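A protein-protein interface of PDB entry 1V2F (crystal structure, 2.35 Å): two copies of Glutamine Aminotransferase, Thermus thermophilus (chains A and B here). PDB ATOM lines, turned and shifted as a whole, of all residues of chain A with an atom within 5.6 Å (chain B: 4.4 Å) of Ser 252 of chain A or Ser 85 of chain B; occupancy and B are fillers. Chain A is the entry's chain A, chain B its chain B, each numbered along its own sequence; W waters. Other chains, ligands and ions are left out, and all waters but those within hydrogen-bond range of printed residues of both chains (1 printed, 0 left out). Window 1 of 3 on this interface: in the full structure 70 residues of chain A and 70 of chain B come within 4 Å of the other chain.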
ATOM      1  N   SER A  85      -8.541 -12.755  16.108  1.00  0.00           N
ATOM      2  CA  SER A  85      -7.430 -12.091  15.455  1.00  0.00           C
ATOM      3  C   SER A  85      -7.001 -12.946  14.260  1.00  0.00           C
ATOM      4  O   SER A  85      -5.939 -13.580  14.273  1.00  0.00           O
ATOM      5  CB  SER A  85      -6.288 -11.924  16.452  1.00  0.00           C
ATOM      6  OG  SER A  85      -6.724 -11.161  17.573  1.00  0.00           O
ATOM      7  N   GLU A  89      -6.297 -17.611  14.397  1.00  0.00           N
ATOM      8  CA  GLU A  89      -6.607 -17.735  15.814  1.00  0.00           C
ATOM      9  C   GLU A  89      -7.914 -18.508  16.008  1.00  0.00           C
ATOM     10  O   GLU A  89      -8.037 -19.305  16.927  1.00  0.00           O
ATOM     11  CB  GLU A  89      -6.725 -16.363  16.471  1.00  0.00           C
ATOM     12  CG  GLU A  89      -6.921 -16.466  17.979  1.00  0.00           C
ATOM     13  CD  GLU A  89      -7.063 -15.122  18.664  1.00  0.00           C
ATOM     14  OE1 GLU A  89      -8.027 -14.396  18.350  1.00  0.00           O
ATOM     15  OE2 GLU A  89      -6.213 -14.796  19.521  1.00  0.00           O
ATOM     16  N   ARG A 248     -10.246 -17.168  23.369  1.00  0.00           N
ATOM     17  CA  ARG A 248      -9.469 -16.197  22.583  1.00  0.00           C
ATOM     18  C   ARG A 248      -9.052 -15.006  23.430  1.00  0.00           C
ATOM     19  O   ARG A 248      -8.156 -14.249  23.084  1.00  0.00           O
ATOM     20  CB  ARG A 248     -10.262 -15.733  21.344  1.00  0.00           C
ATOM     21  CG  ARG A 248     -11.536 -14.930  21.621  1.00  0.00           C
ATOM     22  CD  ARG A 248     -11.262 -13.438  21.772  1.00  0.00           C
ATOM     23  NE  ARG A 248     -10.980 -12.771  20.498  1.00  0.00           N
ATOM     24  CZ  ARG A 248      -9.768 -12.408  20.080  1.00  0.00           C
ATOM     25  NH1 ARG A 248      -8.701 -12.647  20.831  1.00  0.00           N
ATOM     26  NH2 ARG A 248      -9.620 -11.786  18.911  1.00  0.00           N
ATOM     27  N   GLN A 249      -9.703 -14.875  24.570  1.00  0.00           N
ATOM     28  CA  GLN A 249      -9.439 -13.804  25.520  1.00  0.00           C
ATOM     29  C   GLN A 249      -8.014 -13.944  26.103  1.00  0.00           C
ATOM     30  O   GLN A 249      -7.335 -12.947  26.397  1.00  0.00           O
ATOM     31  CB  GLN A 249     -10.498 -13.942  26.596  1.00  0.00           C
ATOM     32  CG  GLN A 249     -10.576 -12.926  27.680  1.00  0.00           C
ATOM     33  CD  GLN A 249     -11.735 -13.266  28.607  1.00  0.00           C
ATOM     34  OE1 GLN A 249     -11.727 -14.311  29.263  1.00  0.00           O
ATOM     35  NE2 GLN A 249     -12.742 -12.409  28.643  1.00  0.00           N
ATOM     36  N   TRP A 250      -7.565 -15.190  26.253  1.00  0.00           N
ATOM     37  CA  TRP A 250      -6.243 -15.481  26.805  1.00  0.00           C
ATOM     38  C   TRP A 250      -5.147 -15.517  25.740  1.00  0.00           C
ATOM     39  O   TRP A 250      -3.971 -15.320  26.046  1.00  0.00           O
ATOM     40  CB  TRP A 250      -6.264 -16.832  27.547  1.00  0.00           C
ATOM     41  CG  TRP A 250      -7.351 -16.937  28.578  1.00  0.00           C
ATOM     42  CD1 TRP A 250      -8.222 -17.974  28.744  1.00  0.00           C
ATOM     43  CD2 TRP A 250      -7.702 -15.960  29.566  1.00  0.00           C
ATOM     44  NE1 TRP A 250      -9.095 -17.705  29.769  1.00  0.00           N
ATOM     45  CE2 TRP A 250      -8.799 -16.474  30.292  1.00  0.00           C
ATOM     46  CE3 TRP A 250      -7.199 -14.699  29.907  1.00  0.00           C
ATOM     47  CZ2 TRP A 250      -9.402 -15.774  31.337  1.00  0.00           C
ATOM     48  CZ3 TRP A 250      -7.799 -13.999  30.948  1.00  0.00           C
ATOM     49  CH2 TRP A 250      -8.891 -14.541  31.651  1.00  0.00           C
ATOM     50  N   THR A 251      -5.517 -15.803  24.497  1.00  0.00           N
ATOM     51  CA  THR A 251      -4.519 -15.852  23.449  1.00  0.00           C
ATOM     52  C   THR A 251      -4.111 -14.446  23.000  1.00  0.00           C
ATOM     53  O   THR A 251      -2.929 -14.122  23.001  1.00  0.00           O
ATOM     54  CB  THR A 251      -5.005 -16.685  22.262  1.00  0.00           C
ATOM     55  OG1 THR A 251      -6.315 -16.251  21.867  1.00  0.00           O
ATOM     56  CG2 THR A 251      -5.035 -18.156  22.648  1.00  0.00           C
ATOM     57  N   SER A 252      -5.070 -13.602  22.630  1.00  0.00           N
ATOM     58  CA  SER A 252      -4.711 -12.242  22.221  1.00  0.00           C
ATOM     59  C   SER A 252      -5.658 -11.187  22.786  1.00  0.00           C
ATOM     60  O   SER A 252      -5.508  -9.999  22.507  1.00  0.00           O
ATOM     61  CB  SER A 252      -4.640 -12.138  20.689  1.00  0.00           C
ATOM     62  OG  SER A 252      -5.901 -12.323  20.075  1.00  0.00           O
ATOM     63  N   PHE A 253      -6.620 -11.640  23.591  1.00  0.00           N
ATOM     64  CA  PHE A 253      -7.627 -10.796  24.244  1.00  0.00           C
ATOM     65  C   PHE A 253      -8.699 -10.269  23.296  1.00  0.00           C
ATOM     66  O   PHE A 253      -9.866 -10.641  23.418  1.00  0.00           O
ATOM     67  CB  PHE A 253      -6.983  -9.619  24.984  1.00  0.00           C
ATOM     68  CG  PHE A 253      -7.955  -8.837  25.839  1.00  0.00           C
ATOM     69  CD1 PHE A 253      -8.476  -9.389  27.012  1.00  0.00           C
ATOM     70  CD2 PHE A 253      -8.377  -7.565  25.459  1.00  0.00           C
ATOM     71  CE1 PHE A 253      -9.402  -8.685  27.792  1.00  0.00           C
ATOM     72  CE2 PHE A 253      -9.305  -6.851  26.230  1.00  0.00           C
ATOM     73  CZ  PHE A 253      -9.817  -7.416  27.399  1.00  0.00           C
ATOM     74  N   SER A 254      -8.310  -9.409  22.356  1.00  0.00           N
ATOM     75  CA  SER A 254      -9.252  -8.852  21.398  1.00  0.00           C
ATOM     76  C   SER A 254      -8.559  -8.450  20.097  1.00  0.00           C
ATOM     77  O   SER A 254      -7.362  -8.189  20.087  1.00  0.00           O
ATOM     78  CB  SER A 254      -9.952  -7.637  22.003  1.00  0.00           C
ATOM     79  OG  SER A 254     -10.948  -7.155  21.120  1.00  0.00           O
ATOM     80  N   ALA A 255      -9.320  -8.397  19.008  1.00  0.00           N
ATOM     81  CA  ALA A 255      -8.787  -8.038  17.693  1.00  0.00           C
ATOM     82  C   ALA A 255      -8.575  -6.526  17.584  1.00  0.00           C
ATOM     83  O   ALA A 255      -9.226  -5.763  18.283  1.00  0.00           O
ATOM     84  CB  ALA A 255      -9.738  -8.533  16.598  1.00  0.00           C
ATOM     85  N   THR B  84       4.519  -9.743  19.010  1.00  0.00           N
ATOM     86  CA  THR B  84       3.298 -10.476  19.298  1.00  0.00           C
ATOM     87  C   THR B  84       2.069  -9.583  19.145  1.00  0.00           C
ATOM     88  O   THR B  84       2.185  -8.359  19.144  1.00  0.00           O
ATOM     89  CB  THR B  84       3.323 -11.013  20.741  1.00  0.00           C
ATOM     90  OG1 THR B  84       3.557  -9.926  21.644  1.00  0.00           O
ATOM     91  CG2 THR B  84       4.420 -12.039  20.909  1.00  0.00           C
ATOM     92  N   SER B  85       0.895 -10.204  19.030  1.00  0.00           N
ATOM     93  CA  SER B  85      -0.355  -9.464  18.894  1.00  0.00           C
ATOM     94  C   SER B  85      -0.765  -9.016  20.290  1.00  0.00           C
ATOM     95  O   SER B  85      -1.688  -9.582  20.888  1.00  0.00           O
ATOM     96  CB  SER B  85      -1.436 -10.364  18.295  1.00  0.00           C
ATOM     97  OG  SER B  85      -1.021 -10.903  17.047  1.00  0.00           O
ATOM     98  N   GLY B  86      -0.074  -7.998  20.801  1.00  0.00           N
ATOM     99  CA  GLY B  86      -0.349  -7.510  22.139  1.00  0.00           C
ATOM    100  C   GLY B  86       0.483  -8.298  23.147  1.00  0.00           C
ATOM    101  O   GLY B  86       0.915  -9.416  22.857  1.00  0.00           O
ATOM    102  N   THR B  88      -0.532  -9.657  25.722  1.00  0.00           N
ATOM    103  CA  THR B  88      -1.328 -10.801  26.132  1.00  0.00           C
ATOM    104  C   THR B  88      -0.899 -12.052  25.387  1.00  0.00           C
ATOM    105  O   THR B  88      -0.874 -13.135  25.963  1.00  0.00           O
ATOM    106  CB  THR B  88      -2.836 -10.562  25.887  1.00  0.00           C
ATOM    107  OG1 THR B  88      -3.298  -9.523  26.758  1.00  0.00           O
ATOM    108  CG2 THR B  88      -3.632 -11.825  26.166  1.00  0.00           C
ATOM    109  N   GLU B  89      -0.564 -11.917  24.107  1.00  0.00           N
ATOM    110  CA  GLU B  89      -0.148 -13.089  23.353  1.00  0.00           C
ATOM    111  C   GLU B  89       1.264 -13.488  23.759  1.00  0.00           C
ATOM    112  O   GLU B  89       1.600 -14.671  23.785  1.00  0.00           O
ATOM    113  CB  GLU B  89      -0.204 -12.835  21.852  1.00  0.00           C
ATOM    114  CG  GLU B  89       0.175 -14.058  21.036  1.00  0.00           C
ATOM    115  CD  GLU B  89       0.019 -13.853  19.541  1.00  0.00           C
ATOM    116  OE1 GLU B  89       0.696 -12.963  18.981  1.00  0.00           O
ATOM    117  OE2 GLU B  89      -0.781 -14.586  18.927  1.00  0.00           O
ATOM    118  N   ARG B 230      -3.118  -3.937  19.503  1.00  0.00           N
ATOM    119  CA  ARG B 230      -2.627  -5.308  19.630  1.00  0.00           C
ATOM    120  C   ARG B 230      -1.221  -5.541  19.036  1.00  0.00           C
ATOM    121  O   ARG B 230      -1.018  -6.397  18.179  1.00  0.00           O
ATOM    122  CB  ARG B 230      -3.634  -6.286  19.002  1.00  0.00           C
ATOM    123  CG  ARG B 230      -5.118  -5.894  19.171  1.00  0.00           C
ATOM    124  CD  ARG B 230      -5.493  -5.587  20.618  1.00  0.00           C
ATOM    125  NE  ARG B 230      -5.186  -6.725  21.478  1.00  0.00           N
ATOM    126  CZ  ARG B 230      -4.522  -6.633  22.623  1.00  0.00           C
ATOM    127  NH1 ARG B 230      -4.099  -5.454  23.057  1.00  0.00           N
ATOM    128  NH2 ARG B 230      -4.256  -7.731  23.319  1.00  0.00           N
ATOM    129  N   VAL B 231      -0.255  -4.762  19.497  1.00  0.00           N
ATOM    130  CA  VAL B 231       1.120  -4.917  19.059  1.00  0.00           C
ATOM    131  C   VAL B 231       1.943  -4.985  20.337  1.00  0.00           C
ATOM    132  O   VAL B 231       1.963  -4.033  21.123  1.00  0.00           O
ATOM    133  CB  VAL B 231       1.620  -3.720  18.211  1.00  0.00           C
ATOM    134  CG1 VAL B 231       3.121  -3.879  17.935  1.00  0.00           C
ATOM    135  CG2 VAL B 231       0.847  -3.645  16.896  1.00  0.00           C
ATOM    136  N   ARG B 248       3.876 -18.354  18.270  1.00  0.00           N
ATOM    137  CA  ARG B 248       2.868 -17.316  17.982  1.00  0.00           C
ATOM    138  C   ARG B 248       2.389 -17.436  16.536  1.00  0.00           C
ATOM    139  O   ARG B 248       1.344 -16.915  16.156  1.00  0.00           O
ATOM    140  CB  ARG B 248       3.432 -15.911  18.235  1.00  0.00           C
ATOM    141  CG  ARG B 248       4.606 -15.519  17.350  1.00  0.00           C
ATOM    142  CD  ARG B 248       4.174 -14.851  16.050  1.00  0.00           C
ATOM    143  NE  ARG B 248       3.665 -13.492  16.251  1.00  0.00           N
ATOM    144  CZ  ARG B 248       2.376 -13.150  16.213  1.00  0.00           C
ATOM    145  NH1 ARG B 248       1.445 -14.076  15.983  1.00  0.00           N
ATOM    146  NH2 ARG B 248       2.015 -11.876  16.389  1.00  0.00           N
ATOM    147  N   SER B 252      -1.837 -16.536  16.136  1.00  0.00           N
ATOM    148  CA  SER B 252      -2.450 -15.477  15.341  1.00  0.00           C
ATOM    149  C   SER B 252      -1.584 -15.150  14.116  1.00  0.00           C
ATOM    150  O   SER B 252      -1.821 -14.167  13.416  1.00  0.00           O
ATOM    151  CB  SER B 252      -2.674 -14.227  16.196  1.00  0.00           C
ATOM    152  OG  SER B 252      -1.452 -13.615  16.563  1.00  0.00           O
ATOM    153  N   SER B 254       0.689 -13.478  12.786  1.00  0.00           N
ATOM    154  CA  SER B 254       1.492 -12.252  12.850  1.00  0.00           C
ATOM    155  C   SER B 254       0.636 -11.076  13.317  1.00  0.00           C
ATOM    156  O   SER B 254      -0.573 -11.105  13.159  1.00  0.00           O
ATOM    157  CB  SER B 254       2.085 -11.944  11.465  1.00  0.00           C
ATOM    158  OG  SER B 254       3.048 -10.907  11.540  1.00  0.00           O
ATOM    159  N   ALA B 255       1.259 -10.043  13.883  1.00  0.00           N
ATOM    160  CA  ALA B 255       0.517  -8.872  14.358  1.00  0.00           C
ATOM    161  C   ALA B 255       0.068  -7.990  13.174  1.00  0.00           C
ATOM    162  O   ALA B 255       0.646  -8.064  12.092  1.00  0.00           O
ATOM    163  CB  ALA B 255       1.379  -8.069  15.341  1.00  0.00           C
HETATM  164  O   HOH W   1      -2.505 -14.279  27.830  1.00  0.00           O
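The backbone NH of Ser 85 of chain A is in hydrogen-bond range of the side-chain carboxylate of Glu 89 of chain A (2.8 Å). OG of Ser 252 of chain A lies within hydrogen-bond range of OG of Ser 85 of chain A, at 2.9 Å. OG1 of Thr 251 of chain A is in hydrogen-bond range of O of Arg 248 of chain A (3.0 Å). The side-chain hydroxyl of Ser 252 of chain A is in hydrogen-bond range of the guanidinium group of Arg 248 of chain A (2.9 Å). The backbone carbonyl oxygen of Arg 248 of chain A sits at hydrogen-bond distance from the backbone NH of Phe 253 of chain A (3.1 Å). OG of Ser 252 of chain B lies within hydrogen-bond range of NH1 of Arg 248 of chain B, 3.0 Å away.
Of the 11 printed residues of chain B, 5 touch a printed residue of chain A. Printed residues of chain B that touch a printed residue of chain A: Ser 85, Thr 88, Glu 89, Arg 230 and Ser 252. Among the printed residues, no Asp or Glu carboxylate lies within 4 Å of a Lys or Arg side-chain nitrogen of the other chain.
Ser 85 of chain A touches Ser 252 of chain B, and with the chains exchanged Ser 252 of chain A touches Ser 85 of chain B. 6 positions are printed for both chains. Of the 12 pairs that touch across the chains among the printed residues, 2 have their exchanged pair printed and touching as well.
Water W1 lies within hydrogen-bond range of O of Trp 250 of chain A (2.5 Å) and O of Thr 88 of chain B (2.7 Å).
Ser 85 of chain A touches Ser 252 of chain B (O to CB, 3.8 Å). CG2 of Thr 88 of chain B touches O of Gln 249 of chain A, 3.9 Å away. Trp 250 of chain A touches Thr 88 of chain B (O to CG2, 3.5 Å). Thr 251 of chain A touches Thr 88 of chain B (O to O, 3.7 Å). CB of Ser 252 of chain A touches O of Ser 85 of chain B, at 3.9 Å. Ser 252 of chain A touches Thr 88 of chain B. Thr 88 of chain B touches Phe 253 of chain A (CG2 to N, 3.9 Å). NH2 of Arg 230 of chain B touches CB of Phe 253 of chain A (3.7 Å). Ala 255 of chain A touches Arg 230 of chain B (C to CG, 3.9 Å).
The backbone carbonyl oxygen of Thr 251 of chain A lies close to the backbone NH of Glu 89 of chain B (3.4 Å). The guanidinium group (NH2) of Arg 230 of chain B is in hydrogen-bond range of the backbone carbonyl oxygen (O) of Ser 252 of chain A (2.7 Å). The backbone carbonyl oxygen of Ser 254 of chain A lies within hydrogen-bond range of the guanidinium group of Arg 230 of chain B, at 3.0 Å.
Ser 85 of chain B touches just one residue of chain A: Ser 252 (3.9 Å). Printed residues of chain A within 4 Å of Glu 89 of chain B: Thr 251 (3.0 Å). Of the printed residues of chain B, Ser 254 of chain A touches Arg 230. Arg 248 of chain B touches none of the printed residues of chain A.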
